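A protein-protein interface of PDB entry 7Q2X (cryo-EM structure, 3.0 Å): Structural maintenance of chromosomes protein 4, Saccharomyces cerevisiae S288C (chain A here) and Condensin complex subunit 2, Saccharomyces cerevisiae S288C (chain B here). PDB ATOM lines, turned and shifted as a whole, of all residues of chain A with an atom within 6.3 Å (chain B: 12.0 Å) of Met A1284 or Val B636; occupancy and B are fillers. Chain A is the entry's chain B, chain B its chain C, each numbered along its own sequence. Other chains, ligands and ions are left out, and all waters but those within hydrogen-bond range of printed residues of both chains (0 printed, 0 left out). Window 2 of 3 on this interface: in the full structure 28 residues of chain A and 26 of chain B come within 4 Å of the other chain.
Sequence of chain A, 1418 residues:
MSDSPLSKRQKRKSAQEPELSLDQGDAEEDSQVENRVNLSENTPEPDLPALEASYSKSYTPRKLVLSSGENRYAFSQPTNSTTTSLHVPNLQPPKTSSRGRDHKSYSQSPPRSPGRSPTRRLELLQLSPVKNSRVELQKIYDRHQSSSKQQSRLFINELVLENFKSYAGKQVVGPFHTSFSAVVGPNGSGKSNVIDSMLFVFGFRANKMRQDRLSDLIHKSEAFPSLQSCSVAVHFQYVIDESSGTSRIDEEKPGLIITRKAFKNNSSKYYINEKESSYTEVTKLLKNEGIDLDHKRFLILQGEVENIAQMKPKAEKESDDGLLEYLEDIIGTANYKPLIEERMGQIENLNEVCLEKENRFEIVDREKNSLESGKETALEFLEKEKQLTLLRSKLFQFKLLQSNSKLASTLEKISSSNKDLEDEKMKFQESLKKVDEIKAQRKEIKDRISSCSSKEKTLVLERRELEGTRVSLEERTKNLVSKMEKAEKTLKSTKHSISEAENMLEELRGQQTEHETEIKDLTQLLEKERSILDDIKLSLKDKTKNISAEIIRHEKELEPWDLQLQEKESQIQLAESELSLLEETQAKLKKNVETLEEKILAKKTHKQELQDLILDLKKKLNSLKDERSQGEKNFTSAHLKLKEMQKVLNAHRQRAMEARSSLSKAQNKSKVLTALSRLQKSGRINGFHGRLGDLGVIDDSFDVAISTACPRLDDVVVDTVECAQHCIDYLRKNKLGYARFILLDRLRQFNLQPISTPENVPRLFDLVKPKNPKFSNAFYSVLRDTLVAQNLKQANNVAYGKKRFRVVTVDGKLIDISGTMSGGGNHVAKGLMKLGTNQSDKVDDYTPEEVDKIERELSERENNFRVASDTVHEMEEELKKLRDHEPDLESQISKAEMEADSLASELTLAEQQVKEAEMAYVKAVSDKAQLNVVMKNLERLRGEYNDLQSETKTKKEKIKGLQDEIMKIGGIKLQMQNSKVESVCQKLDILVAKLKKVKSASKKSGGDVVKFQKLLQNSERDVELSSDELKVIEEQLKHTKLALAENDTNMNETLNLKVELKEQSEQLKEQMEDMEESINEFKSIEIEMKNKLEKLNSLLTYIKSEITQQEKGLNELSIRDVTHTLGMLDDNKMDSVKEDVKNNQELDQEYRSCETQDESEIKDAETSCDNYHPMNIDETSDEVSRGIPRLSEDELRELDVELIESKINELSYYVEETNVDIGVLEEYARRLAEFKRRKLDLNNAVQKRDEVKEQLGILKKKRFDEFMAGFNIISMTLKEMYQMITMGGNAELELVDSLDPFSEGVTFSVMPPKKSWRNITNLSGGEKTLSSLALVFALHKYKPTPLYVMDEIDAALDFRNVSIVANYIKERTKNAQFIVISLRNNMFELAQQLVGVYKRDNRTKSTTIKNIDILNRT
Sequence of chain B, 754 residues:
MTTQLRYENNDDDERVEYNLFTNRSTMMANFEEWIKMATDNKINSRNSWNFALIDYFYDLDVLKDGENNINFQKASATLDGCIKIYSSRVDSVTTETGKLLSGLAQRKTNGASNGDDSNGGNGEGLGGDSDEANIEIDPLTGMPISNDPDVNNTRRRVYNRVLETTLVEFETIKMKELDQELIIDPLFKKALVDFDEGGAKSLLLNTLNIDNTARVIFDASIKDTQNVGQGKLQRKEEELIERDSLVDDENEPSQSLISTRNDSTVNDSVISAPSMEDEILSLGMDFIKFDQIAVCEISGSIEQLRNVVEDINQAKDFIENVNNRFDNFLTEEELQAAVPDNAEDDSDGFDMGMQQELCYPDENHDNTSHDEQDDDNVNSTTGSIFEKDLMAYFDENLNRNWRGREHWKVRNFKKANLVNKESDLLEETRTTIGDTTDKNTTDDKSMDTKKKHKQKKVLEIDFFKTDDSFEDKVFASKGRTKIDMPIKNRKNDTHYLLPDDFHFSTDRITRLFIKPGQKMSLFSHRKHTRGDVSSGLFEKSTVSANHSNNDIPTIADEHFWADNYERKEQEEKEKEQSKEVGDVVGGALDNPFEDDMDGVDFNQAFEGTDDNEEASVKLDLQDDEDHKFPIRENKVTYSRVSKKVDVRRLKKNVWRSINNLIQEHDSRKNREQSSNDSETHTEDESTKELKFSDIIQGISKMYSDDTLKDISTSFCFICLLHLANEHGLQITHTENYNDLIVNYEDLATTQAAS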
ATOM      1  N   LYS A1279     -35.219  -5.400   5.168  1.00  0.00           N
ATOM      2  CA  LYS A1279     -35.588  -5.955   6.465  1.00  0.00           C
ATOM      3  C   LYS A1279     -35.265  -7.442   6.527  1.00  0.00           C
ATOM      4  O   LYS A1279     -34.697  -7.926   7.514  1.00  0.00           O
ATOM      5  CB  LYS A1279     -37.073  -5.710   6.735  1.00  0.00           C
ATOM      6  CG  LYS A1279     -37.533  -6.137   8.119  1.00  0.00           C
ATOM      7  CD  LYS A1279     -39.029  -5.925   8.289  1.00  0.00           C
ATOM      8  CE  LYS A1279     -39.365  -4.450   8.439  1.00  0.00           C
ATOM      9  NZ  LYS A1279     -40.810  -4.234   8.724  1.00  0.00           N
ATOM     10  N   GLU A1280     -35.601  -8.180   5.464  1.00  0.00           N
ATOM     11  CA  GLU A1280     -35.308  -9.611   5.443  1.00  0.00           C
ATOM     12  C   GLU A1280     -33.806  -9.872   5.505  1.00  0.00           C
ATOM     13  O   GLU A1280     -33.351 -10.750   6.249  1.00  0.00           O
ATOM     14  CB  GLU A1280     -35.915 -10.252   4.195  1.00  0.00           C
ATOM     15  CG  GLU A1280     -36.007 -11.774   4.246  1.00  0.00           C
ATOM     16  CD  GLU A1280     -37.128 -12.279   5.140  1.00  0.00           C
ATOM     17  OE1 GLU A1280     -37.804 -11.454   5.790  1.00  0.00           O
ATOM     18  OE2 GLU A1280     -37.334 -13.510   5.191  1.00  0.00           O
ATOM     19  N   MET A1281     -33.020  -9.115   4.734  1.00  0.00           N
ATOM     20  CA  MET A1281     -31.576  -9.319   4.721  1.00  0.00           C
ATOM     21  C   MET A1281     -30.953  -8.992   6.070  1.00  0.00           C
ATOM     22  O   MET A1281     -30.087  -9.728   6.552  1.00  0.00           O
ATOM     23  CB  MET A1281     -30.932  -8.481   3.617  1.00  0.00           C
ATOM     24  CG  MET A1281     -29.796  -9.191   2.904  1.00  0.00           C
ATOM     25  SD  MET A1281     -30.379 -10.491   1.803  1.00  0.00           S
ATOM     26  CE  MET A1281     -30.706  -9.543   0.324  1.00  0.00           C
ATOM     27  N   TYR A1282     -31.375  -7.889   6.693  1.00  0.00           N
ATOM     28  CA  TYR A1282     -30.844  -7.548   8.008  1.00  0.00           C
ATOM     29  C   TYR A1282     -31.216  -8.606   9.038  1.00  0.00           C
ATOM     30  O   TYR A1282     -30.383  -8.989   9.868  1.00  0.00           O
ATOM     31  CB  TYR A1282     -31.345  -6.171   8.443  1.00  0.00           C
ATOM     32  CG  TYR A1282     -30.552  -5.582   9.586  1.00  0.00           C
ATOM     33  CD1 TYR A1282     -29.306  -5.010   9.368  1.00  0.00           C
ATOM     34  CD2 TYR A1282     -31.041  -5.608  10.884  1.00  0.00           C
ATOM     35  CE1 TYR A1282     -28.573  -4.474  10.407  1.00  0.00           C
ATOM     36  CE2 TYR A1282     -30.315  -5.075  11.932  1.00  0.00           C
ATOM     37  CZ  TYR A1282     -29.082  -4.510  11.687  1.00  0.00           C
ATOM     38  OH  TYR A1282     -28.353  -3.979  12.726  1.00  0.00           O
ATOM     39  N   GLN A1283     -32.456  -9.101   8.987  1.00  0.00           N
ATOM     40  CA  GLN A1283     -32.872 -10.144   9.918  1.00  0.00           C
ATOM     41  C   GLN A1283     -32.041 -11.409   9.741  1.00  0.00           C
ATOM     42  O   GLN A1283     -31.638 -12.036  10.728  1.00  0.00           O
ATOM     43  CB  GLN A1283     -34.357 -10.450   9.730  1.00  0.00           C
ATOM     44  CG  GLN A1283     -34.980 -11.228  10.878  1.00  0.00           C
ATOM     45  CD  GLN A1283     -36.329 -11.817  10.516  1.00  0.00           C
ATOM     46  OE1 GLN A1283     -37.026 -11.307   9.638  1.00  0.00           O
ATOM     47  NE2 GLN A1283     -36.704 -12.897  11.190  1.00  0.00           N
ATOM     48  N   MET A1284     -31.772 -11.803   8.494  1.00  0.00           N
ATOM     49  CA  MET A1284     -31.061 -13.059   8.276  1.00  0.00           C
ATOM     50  C   MET A1284     -29.569 -12.922   8.563  1.00  0.00           C
ATOM     51  O   MET A1284     -28.929 -13.884   9.006  1.00  0.00           O
ATOM     52  CB  MET A1284     -31.306 -13.573   6.853  1.00  0.00           C
ATOM     53  CG  MET A1284     -30.805 -12.683   5.725  1.00  0.00           C
ATOM     54  SD  MET A1284     -29.051 -12.883   5.352  1.00  0.00           S
ATOM     55  CE  MET A1284     -29.052 -14.524   4.636  1.00  0.00           C
ATOM     56  N   ILE A1285     -28.989 -11.742   8.321  1.00  0.00           N
ATOM     57  CA  ILE A1285     -27.550 -11.585   8.508  1.00  0.00           C
ATOM     58  C   ILE A1285     -27.227 -11.269   9.965  1.00  0.00           C
ATOM     59  O   ILE A1285     -26.110 -11.516  10.434  1.00  0.00           O
ATOM     60  CB  ILE A1285     -26.996 -10.507   7.558  1.00  0.00           C
ATOM     61  CG1 ILE A1285     -25.471 -10.592   7.481  1.00  0.00           C
ATOM     62  CG2 ILE A1285     -27.394  -9.116   8.026  1.00  0.00           C
ATOM     63  CD1 ILE A1285     -24.872  -9.792   6.346  1.00  0.00           C
ATOM     64  N   THR A1286     -28.193 -10.725  10.703  1.00  0.00           N
ATOM     65  CA  THR A1286     -27.962 -10.319  12.081  1.00  0.00           C
ATOM     66  C   THR A1286     -28.578 -11.287  13.088  1.00  0.00           C
ATOM     67  O   THR A1286     -28.158 -11.301  14.251  1.00  0.00           O
ATOM     68  CB  THR A1286     -28.512  -8.898  12.286  1.00  0.00           C
ATOM     69  OG1 THR A1286     -27.843  -8.001  11.392  1.00  0.00           O
ATOM     70  CG2 THR A1286     -28.268  -8.403  13.699  1.00  0.00           C
ATOM     71  N   MET A1287     -29.518 -12.132  12.654  1.00  0.00           N
ATOM     72  CA  MET A1287     -30.276 -13.010  13.548  1.00  0.00           C
ATOM     73  C   MET A1287     -31.005 -12.199  14.616  1.00  0.00           C
ATOM     74  O   MET A1287     -31.017 -12.553  15.797  1.00  0.00           O
ATOM     75  CB  MET A1287     -29.381 -14.076  14.187  1.00  0.00           C
ATOM     76  CG  MET A1287     -28.672 -14.973  13.187  1.00  0.00           C
ATOM     77  SD  MET A1287     -26.935 -15.225  13.599  1.00  0.00           S
ATOM     78  CE  MET A1287     -26.175 -13.907  12.660  1.00  0.00           C
ATOM     79  N   GLY A1288     -31.614 -11.106  14.194  1.00  0.00           N
ATOM     80  CA  GLY A1288     -32.314 -10.213  15.096  1.00  0.00           C
ATOM     81  C   GLY A1288     -32.270  -8.792  14.581  1.00  0.00           C
ATOM     82  O   GLY A1288     -31.514  -8.452  13.673  1.00  0.00           O
ATOM     83  N   SER A1363     -16.886 -13.704   9.597  1.00  0.00           N
ATOM     84  CA  SER A1363     -17.213 -15.048   9.132  1.00  0.00           C
ATOM     85  C   SER A1363     -18.618 -15.102   8.545  1.00  0.00           C
ATOM     86  O   SER A1363     -18.852 -15.784   7.542  1.00  0.00           O
ATOM     87  CB  SER A1363     -17.068 -16.049  10.277  1.00  0.00           C
ATOM     88  OG  SER A1363     -17.410 -17.358   9.854  1.00  0.00           O
ATOM     89  N   ILE A1364     -19.566 -14.392   9.161  1.00  0.00           N
ATOM     90  CA  ILE A1364     -20.936 -14.373   8.651  1.00  0.00           C
ATOM     91  C   ILE A1364     -20.974 -13.769   7.253  1.00  0.00           C
ATOM     92  O   ILE A1364     -21.608 -14.309   6.337  1.00  0.00           O
ATOM     93  CB  ILE A1364     -21.859 -13.613   9.620  1.00  0.00           C
ATOM     94  CG1 ILE A1364     -22.153 -14.462  10.857  1.00  0.00           C
ATOM     95  CG2 ILE A1364     -23.155 -13.217   8.930  1.00  0.00           C
ATOM     96  CD1 ILE A1364     -22.554 -13.654  12.069  1.00  0.00           C
ATOM     97  N   VAL A1365     -20.287 -12.639   7.065  1.00  0.00           N
ATOM     98  CA  VAL A1365     -20.267 -11.985   5.757  1.00  0.00           C
ATOM     99  C   VAL A1365     -19.578 -12.871   4.725  1.00  0.00           C
ATOM    100  O   VAL A1365     -20.045 -13.001   3.583  1.00  0.00           O
ATOM    101  CB  VAL A1365     -19.592 -10.604   5.863  1.00  0.00           C
ATOM    102  CG1 VAL A1365     -19.381 -10.004   4.482  1.00  0.00           C
ATOM    103  CG2 VAL A1365     -20.425  -9.675   6.730  1.00  0.00           C
ATOM    104  N   ASN A1367     -19.316 -16.162   4.722  1.00  0.00           N
ATOM    105  CA  ASN A1367     -20.183 -17.289   4.396  1.00  0.00           C
ATOM    106  C   ASN A1367     -21.361 -16.854   3.534  1.00  0.00           C
ATOM    107  O   ASN A1367     -21.790 -17.596   2.643  1.00  0.00           O
ATOM    108  CB  ASN A1367     -20.671 -17.963   5.676  1.00  0.00           C
ATOM    109  CG  ASN A1367     -19.721 -19.036   6.167  1.00  0.00           C
ATOM    110  OD1 ASN A1367     -19.028 -18.858   7.169  1.00  0.00           O
ATOM    111  ND2 ASN A1367     -19.684 -20.160   5.461  1.00  0.00           N
ATOM    112  N   TYR A1368     -21.905 -15.662   3.791  1.00  0.00           N
ATOM    113  CA  TYR A1368     -22.991 -15.154   2.959  1.00  0.00           C
ATOM    114  C   TYR A1368     -22.530 -14.956   1.522  1.00  0.00           C
ATOM    115  O   TYR A1368     -23.258 -15.285   0.577  1.00  0.00           O
ATOM    116  CB  TYR A1368     -23.530 -13.844   3.537  1.00  0.00           C
ATOM    117  CG  TYR A1368     -24.633 -13.217   2.713  1.00  0.00           C
ATOM    118  CD1 TYR A1368     -25.961 -13.561   2.922  1.00  0.00           C
ATOM    119  CD2 TYR A1368     -24.347 -12.278   1.730  1.00  0.00           C
ATOM    120  CE1 TYR A1368     -26.973 -12.991   2.172  1.00  0.00           C
ATOM    121  CE2 TYR A1368     -25.352 -11.706   0.975  1.00  0.00           C
ATOM    122  CZ  TYR A1368     -26.663 -12.064   1.201  1.00  0.00           C
ATOM    123  OH  TYR A1368     -27.666 -11.494   0.454  1.00  0.00           O
ATOM    124  N   GLU A1371     -22.070 -18.565  -0.080  1.00  0.00           N
ATOM    125  CA  GLU A1371     -23.231 -19.405  -0.346  1.00  0.00           C
ATOM    126  C   GLU A1371     -24.356 -18.674  -1.069  1.00  0.00           C
ATOM    127  O   GLU A1371     -24.806 -19.124  -2.126  1.00  0.00           O
ATOM    128  CB  GLU A1371     -23.758 -19.995   0.968  1.00  0.00           C
ATOM    129  CG  GLU A1371     -22.811 -20.987   1.627  1.00  0.00           C
ATOM    130  CD  GLU A1371     -23.344 -21.516   2.944  1.00  0.00           C
ATOM    131  OE1 GLU A1371     -24.400 -21.028   3.399  1.00  0.00           O
ATOM    132  OE2 GLU A1371     -22.706 -22.419   3.525  1.00  0.00           O
ATOM    133  N   ARG A1372     -24.823 -17.552  -0.521  1.00  0.00           N
ATOM    134  CA  ARG A1372     -26.032 -16.918  -1.029  1.00  0.00           C
ATOM    135  C   ARG A1372     -25.784 -16.025  -2.241  1.00  0.00           C
ATOM    136  O   ARG A1372     -26.751 -15.599  -2.882  1.00  0.00           O
ATOM    137  CB  ARG A1372     -26.699 -16.112   0.091  1.00  0.00           C
ATOM    138  CG  ARG A1372     -28.168 -15.794  -0.146  1.00  0.00           C
ATOM    139  CD  ARG A1372     -28.956 -15.742   1.158  1.00  0.00           C
ATOM    140  NE  ARG A1372     -29.158 -17.067   1.737  1.00  0.00           N
ATOM    141  CZ  ARG A1372     -28.380 -17.615   2.661  1.00  0.00           C
ATOM    142  NH1 ARG A1372     -27.332 -16.974   3.153  1.00  0.00           N
ATOM    143  NH2 ARG A1372     -28.663 -18.836   3.106  1.00  0.00           N
ATOM    144  N   LYS B 635     -28.941 -19.645  10.614  1.00  0.00           N
ATOM    145  CA  LYS B 635     -29.185 -19.650   9.177  1.00  0.00           C
ATOM    146  C   LYS B 635     -27.874 -19.633   8.398  1.00  0.00           C
ATOM    147  O   LYS B 635     -27.648 -20.470   7.525  1.00  0.00           O
ATOM    148  CB  LYS B 635     -30.052 -18.455   8.775  1.00  0.00           C
ATOM    149  N   VAL B 636     -27.013 -18.674   8.722  1.00  0.00           N
ATOM    150  CA  VAL B 636     -25.717 -18.534   8.068  1.00  0.00           C
ATOM    151  C   VAL B 636     -24.646 -19.130   8.970  1.00  0.00           C
ATOM    152  O   VAL B 636     -24.545 -18.774  10.151  1.00  0.00           O
ATOM    153  CB  VAL B 636     -25.417 -17.060   7.752  1.00  0.00           C
ATOM    154  CG1 VAL B 636     -24.026 -16.918   7.152  1.00  0.00           C
ATOM    155  CG2 VAL B 636     -26.471 -16.493   6.814  1.00  0.00           C
ATOM    156  N   THR B 637     -23.851 -20.042   8.418  1.00  0.00           N
ATOM    157  CA  THR B 637     -22.779 -20.666   9.182  1.00  0.00           C
ATOM    158  C   THR B 637     -21.696 -19.645   9.508  1.00  0.00           C
ATOM    159  O   THR B 637     -21.414 -18.741   8.718  1.00  0.00           O
ATOM    160  CB  THR B 637     -22.183 -21.837   8.397  1.00  0.00           C
ATOM    161  OG1 THR B 637     -23.241 -22.663   7.894  1.00  0.00           O
ATOM    162  CG2 THR B 637     -21.279 -22.679   9.288  1.00  0.00           C
ATOM    163  N   TYR B 638     -21.096 -19.783  10.688  1.00  0.00           N
ATOM    164  CA  TYR B 638     -20.007 -18.911  11.098  1.00  0.00           C
ATOM    165  C   TYR B 638     -19.136 -19.641  12.109  1.00  0.00           C
ATOM    166  O   TYR B 638     -19.542 -20.647  12.698  1.00  0.00           O
ATOM    167  CB  TYR B 638     -20.523 -17.592  11.687  1.00  0.00           C
ATOM    168  CG  TYR B 638     -21.499 -17.764  12.830  1.00  0.00           C
ATOM    169  CD1 TYR B 638     -22.862 -17.867  12.596  1.00  0.00           C
ATOM    170  CD2 TYR B 638     -21.054 -17.819  14.144  1.00  0.00           C
ATOM    171  CE1 TYR B 638     -23.756 -18.023  13.637  1.00  0.00           C
ATOM    172  CE2 TYR B 638     -21.939 -17.973  15.191  1.00  0.00           C
ATOM    173  CZ  TYR B 638     -23.289 -18.075  14.933  1.00  0.00           C
ATOM    174  OH  TYR B 638     -24.175 -18.229  15.974  1.00  0.00           O
ATOM    175  N   SER B 639     -17.928 -19.119  12.303  1.00  0.00           N
ATOM    176  CA  SER B 639     -16.993 -19.689  13.265  1.00  0.00           C
ATOM    177  C   SER B 639     -17.392 -19.262  14.672  1.00  0.00           C
ATOM    178  O   SER B 639     -17.451 -18.066  14.972  1.00  0.00           O
ATOM    179  CB  SER B 639     -15.567 -19.245  12.948  1.00  0.00           C
ATOM    180  OG  SER B 639     -15.098 -19.850  11.756  1.00  0.00           O
ATOM    181  N   ARG B 640     -17.675 -20.241  15.532  1.00  0.00           N
ATOM    182  CA  ARG B 640     -18.066 -19.949  16.906  1.00  0.00           C
ATOM    183  C   ARG B 640     -16.886 -19.565  17.789  1.00  0.00           C
ATOM    184  O   ARG B 640     -17.082 -18.858  18.784  1.00  0.00           O
ATOM    185  CB  ARG B 640     -18.790 -21.152  17.515  1.00  0.00           C
ATOM    186  CG  ARG B 640     -20.291 -21.166  17.269  1.00  0.00           C
ATOM    187  CD  ARG B 640     -20.623 -21.746  15.904  1.00  0.00           C
ATOM    188  NE  ARG B 640     -20.237 -23.148  15.800  1.00  0.00           N
ATOM    189  CZ  ARG B 640     -20.202 -23.833  14.665  1.00  0.00           C
ATOM    190  NH1 ARG B 640     -20.525 -23.274  13.510  1.00  0.00           N
ATOM    191  NH2 ARG B 640     -19.834 -25.110  14.688  1.00  0.00           N
ATOM    192  N   VAL B 641     -15.677 -20.008  17.456  1.00  0.00           N
ATOM    193  CA  VAL B 641     -14.493 -19.766  18.272  1.00  0.00           C
ATOM    194  C   VAL B 641     -13.430 -19.094  17.413  1.00  0.00           C
ATOM    195  O   VAL B 641     -13.276 -19.414  16.230  1.00  0.00           O
ATOM    196  CB  VAL B 641     -13.960 -21.074  18.899  1.00  0.00           C
ATOM    197  CG1 VAL B 641     -13.516 -22.057  17.823  1.00  0.00           C
ATOM    198  CG2 VAL B 641     -12.827 -20.783  19.874  1.00  0.00           C
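Of the 7 printed residues of chain B, 4 touch a printed residue of chain A.
Hydrophobic or aromatic side chains of chain B that line the printed part of chain A: Val B636 and Tyr B638.
Among the printed residues, 8 pairs touch across the chains.
Val B636 touches just these residues of chain A: Met A1284 (3.9 Å), Ile A1364 (3.6 Å), Asn A1367 (3.8 Å) and Arg A1372 (3.8 Å).
No residue of chain B comes within 4 Å of Met A1281.
No residue of chain B comes within 4 Å of Gln A1283.
No residue of chain B comes within 4 Å of Ile A1285.
No residue of chain B comes within 4 Å of Gly A1288.
Ile A1364 touches just these residues of chain B: Val B636 and Tyr B638.
No residue of chain B comes within 4 Å of Tyr A1368.
Printed residues of chain A within 4 Å of Ser B639: Ser A1363.
Printed residues of chain A within 4 Å of Thr B637: Asn A1367 (2.8 Å).
Val A1365 touches none of the printed residues of chain B.
The backbone carbonyl oxygen (O) of Tyr B638 sits at hydrogen-bond distance from the guanidinium group (NH1) of Arg B640 (2.9 Å).
The side-chain amide oxygen (OD1) of Asn A1367 lies close to the backbone carbonyl oxygen (O) of Ser A1363 (3.1 Å).
Met A1284 touches Val B636 (CE to CG2, 3.9 Å).
Tyr B638 touches Ser A1363.
Ile A1364 touches Val B636 (O to CG1, 3.6 Å).
Ile A1364 touches Tyr B638 (CG1 to CB, 3.6 Å).
CB of Asn A1367 touches CG1 of Val B636, at 3.8 Å.
NH1 of Arg A1372 touches CG2 of Val B636, at 3.8 Å.
OG of Ser A1363 sits at hydrogen-bond distance from N of Ser B639 (3.1 Å).
The backbone carbonyl oxygen (O) of Thr B637 lies close to the side-chain amide oxygen (OD1) of Asn A1367.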
